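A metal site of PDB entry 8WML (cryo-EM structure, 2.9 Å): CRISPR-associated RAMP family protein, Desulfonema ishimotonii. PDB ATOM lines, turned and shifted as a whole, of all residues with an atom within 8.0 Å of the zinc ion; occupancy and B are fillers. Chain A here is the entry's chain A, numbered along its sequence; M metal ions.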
ATOM      1  N   ARG A 684     -25.701 -19.786  -2.714  1.00  0.00           N
ATOM      2  CA  ARG A 684     -24.497 -20.613  -2.651  1.00  0.00           C
ATOM      3  C   ARG A 684     -24.856 -22.086  -2.458  1.00  0.00           C
ATOM      4  O   ARG A 684     -24.284 -22.959  -3.116  1.00  0.00           O
ATOM      5  CB  ARG A 684     -23.601 -20.124  -1.516  1.00  0.00           C
ATOM      6  CG  ARG A 684     -22.311 -20.908  -1.356  1.00  0.00           C
ATOM      7  CD  ARG A 684     -21.373 -20.204  -0.397  1.00  0.00           C
ATOM      8  NE  ARG A 684     -20.063 -20.843  -0.359  1.00  0.00           N
ATOM      9  CZ  ARG A 684     -19.776 -21.937   0.352  1.00  0.00           C
ATOM     10  NH1 ARG A 684     -20.679 -22.540   1.091  1.00  0.00           N
ATOM     11  NH2 ARG A 684     -18.533 -22.424   0.300  1.00  0.00           N
ATOM     12  N   CYS A 706      -7.272 -24.774  -3.048  1.00  0.00           N
ATOM     13  CA  CYS A 706      -8.403 -25.184  -3.854  1.00  0.00           C
ATOM     14  C   CYS A 706      -8.656 -24.177  -4.968  1.00  0.00           C
ATOM     15  O   CYS A 706      -8.354 -22.996  -4.819  1.00  0.00           O
ATOM     16  CB  CYS A 706      -9.653 -25.348  -2.993  1.00  0.00           C
ATOM     17  SG  CYS A 706     -11.160 -25.765  -3.893  1.00  0.00           S
ATOM     18  N   GLU A 707      -9.165 -24.675  -6.098  1.00  0.00           N
ATOM     19  CA  GLU A 707      -9.446 -23.819  -7.286  1.00  0.00           C
ATOM     20  C   GLU A 707     -10.786 -24.245  -7.880  1.00  0.00           C
ATOM     21  O   GLU A 707     -10.974 -24.046  -9.096  1.00  0.00           O
ATOM     22  CB  GLU A 707      -8.387 -24.080  -8.362  1.00  0.00           C
ATOM     23  CG  GLU A 707      -8.530 -23.203  -9.601  1.00  0.00           C
ATOM     24  CD  GLU A 707      -9.568 -23.627 -10.632  1.00  0.00           C
ATOM     25  OE1 GLU A 707      -9.900 -24.833 -10.682  1.00  0.00           O
ATOM     26  OE2 GLU A 707     -10.033 -22.741 -11.384  1.00  0.00           O
ATOM     27  N   CYS A 708     -11.667 -24.830  -7.065  1.00  0.00           N
ATOM     28  CA  CYS A 708     -12.961 -25.295  -7.529  1.00  0.00           C
ATOM     29  C   CYS A 708     -13.868 -24.124  -7.924  1.00  0.00           C
ATOM     30  O   CYS A 708     -13.578 -22.953  -7.632  1.00  0.00           O
ATOM     31  CB  CYS A 708     -13.645 -26.133  -6.441  1.00  0.00           C
ATOM     32  SG  CYS A 708     -14.085 -25.220  -4.949  1.00  0.00           S
ATOM     33  N   LEU A 709     -14.970 -24.447  -8.602  1.00  0.00           N
ATOM     34  CA  LEU A 709     -15.873 -23.426  -9.131  1.00  0.00           C
ATOM     35  C   LEU A 709     -16.461 -22.580  -8.007  1.00  0.00           C
ATOM     36  O   LEU A 709     -16.551 -21.354  -8.131  1.00  0.00           O
ATOM     37  CB  LEU A 709     -16.974 -24.095  -9.945  1.00  0.00           C
ATOM     38  CG  LEU A 709     -17.907 -23.214 -10.776  1.00  0.00           C
ATOM     39  CD1 LEU A 709     -18.169 -23.859 -12.128  1.00  0.00           C
ATOM     40  CD2 LEU A 709     -19.211 -22.958 -10.051  1.00  0.00           C
ATOM     41  N   LEU A 710     -16.862 -23.228  -6.915  1.00  0.00           N
ATOM     42  CA  LEU A 710     -17.449 -22.497  -5.800  1.00  0.00           C
ATOM     43  C   LEU A 710     -16.448 -21.524  -5.201  1.00  0.00           C
ATOM     44  O   LEU A 710     -16.781 -20.366  -4.924  1.00  0.00           O
ATOM     45  CB  LEU A 710     -17.931 -23.493  -4.731  1.00  0.00           C
ATOM     46  CG  LEU A 710     -19.099 -23.038  -3.844  1.00  0.00           C
ATOM     47  CD1 LEU A 710     -20.404 -23.062  -4.615  1.00  0.00           C
ATOM     48  CD2 LEU A 710     -19.190 -23.924  -2.620  1.00  0.00           C
ATOM     49  N   CYS A 711     -15.207 -21.961  -5.021  1.00  0.00           N
ATOM     50  CA  CYS A 711     -14.181 -21.070  -4.485  1.00  0.00           C
ATOM     51  C   CYS A 711     -13.933 -19.903  -5.435  1.00  0.00           C
ATOM     52  O   CYS A 711     -13.846 -18.754  -4.997  1.00  0.00           O
ATOM     53  CB  CYS A 711     -12.888 -21.839  -4.240  1.00  0.00           C
ATOM     54  SG  CYS A 711     -12.882 -22.802  -2.704  1.00  0.00           S
ATOM     55  N   GLN A 712     -13.835 -20.180  -6.736  1.00  0.00           N
ATOM     56  CA  GLN A 712     -13.535 -19.113  -7.687  1.00  0.00           C
ATOM     57  C   GLN A 712     -14.648 -18.071  -7.721  1.00  0.00           C
ATOM     58  O   GLN A 712     -14.375 -16.873  -7.813  1.00  0.00           O
ATOM     59  CB  GLN A 712     -13.310 -19.686  -9.090  1.00  0.00           C
ATOM     60  CG  GLN A 712     -12.014 -20.464  -9.328  1.00  0.00           C
ATOM     61  CD  GLN A 712     -10.769 -19.794  -8.775  1.00  0.00           C
ATOM     62  OE1 GLN A 712     -10.206 -18.888  -9.396  1.00  0.00           O
ATOM     63  NE2 GLN A 712     -10.336 -20.219  -7.596  1.00  0.00           N
ATOM     64  N   GLY A 715     -15.484 -16.803  -3.583  1.00  0.00           N
ATOM     65  CA  GLY A 715     -14.364 -16.505  -2.713  1.00  0.00           C
ATOM     66  C   GLY A 715     -14.204 -17.561  -1.625  1.00  0.00           C
ATOM     67  O   GLY A 715     -14.987 -18.489  -1.492  1.00  0.00           O
ATOM     68  N   SER A 716     -13.155 -17.384  -0.834  1.00  0.00           N
ATOM     69  CA  SER A 716     -12.844 -18.293   0.269  1.00  0.00           C
ATOM     70  C   SER A 716     -11.979 -17.533   1.273  1.00  0.00           C
ATOM     71  O   SER A 716     -11.835 -16.311   1.191  1.00  0.00           O
ATOM     72  CB  SER A 716     -12.153 -19.559  -0.253  1.00  0.00           C
ATOM     73  OG  SER A 716     -10.856 -19.281  -0.731  1.00  0.00           O
ATOM     74  N   GLU A 719      -8.957 -15.987  -0.706  1.00  0.00           N
ATOM     75  CA  GLU A 719      -9.178 -15.134  -1.872  1.00  0.00           C
ATOM     76  C   GLU A 719     -10.538 -14.472  -1.762  1.00  0.00           C
ATOM     77  O   GLU A 719     -11.471 -15.034  -1.192  1.00  0.00           O
ATOM     78  CB  GLU A 719      -9.070 -15.943  -3.174  1.00  0.00           C
ATOM     79  CG  GLU A 719     -10.246 -16.879  -3.444  1.00  0.00           C
ATOM     80  CD  GLU A 719      -9.806 -18.219  -3.999  1.00  0.00           C
ATOM     81  OE1 GLU A 719      -9.291 -18.263  -5.149  1.00  0.00           O
ATOM     82  OE2 GLU A 719      -9.966 -19.237  -3.301  1.00  0.00           O
HETATM   83 ZN    ZN M   1     -13.103 -25.088  -2.877  1.00  0.00          ZN
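The zinc ion is bound by SG of Cys 706, SG of Cys 708 and SG of Cys 711.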
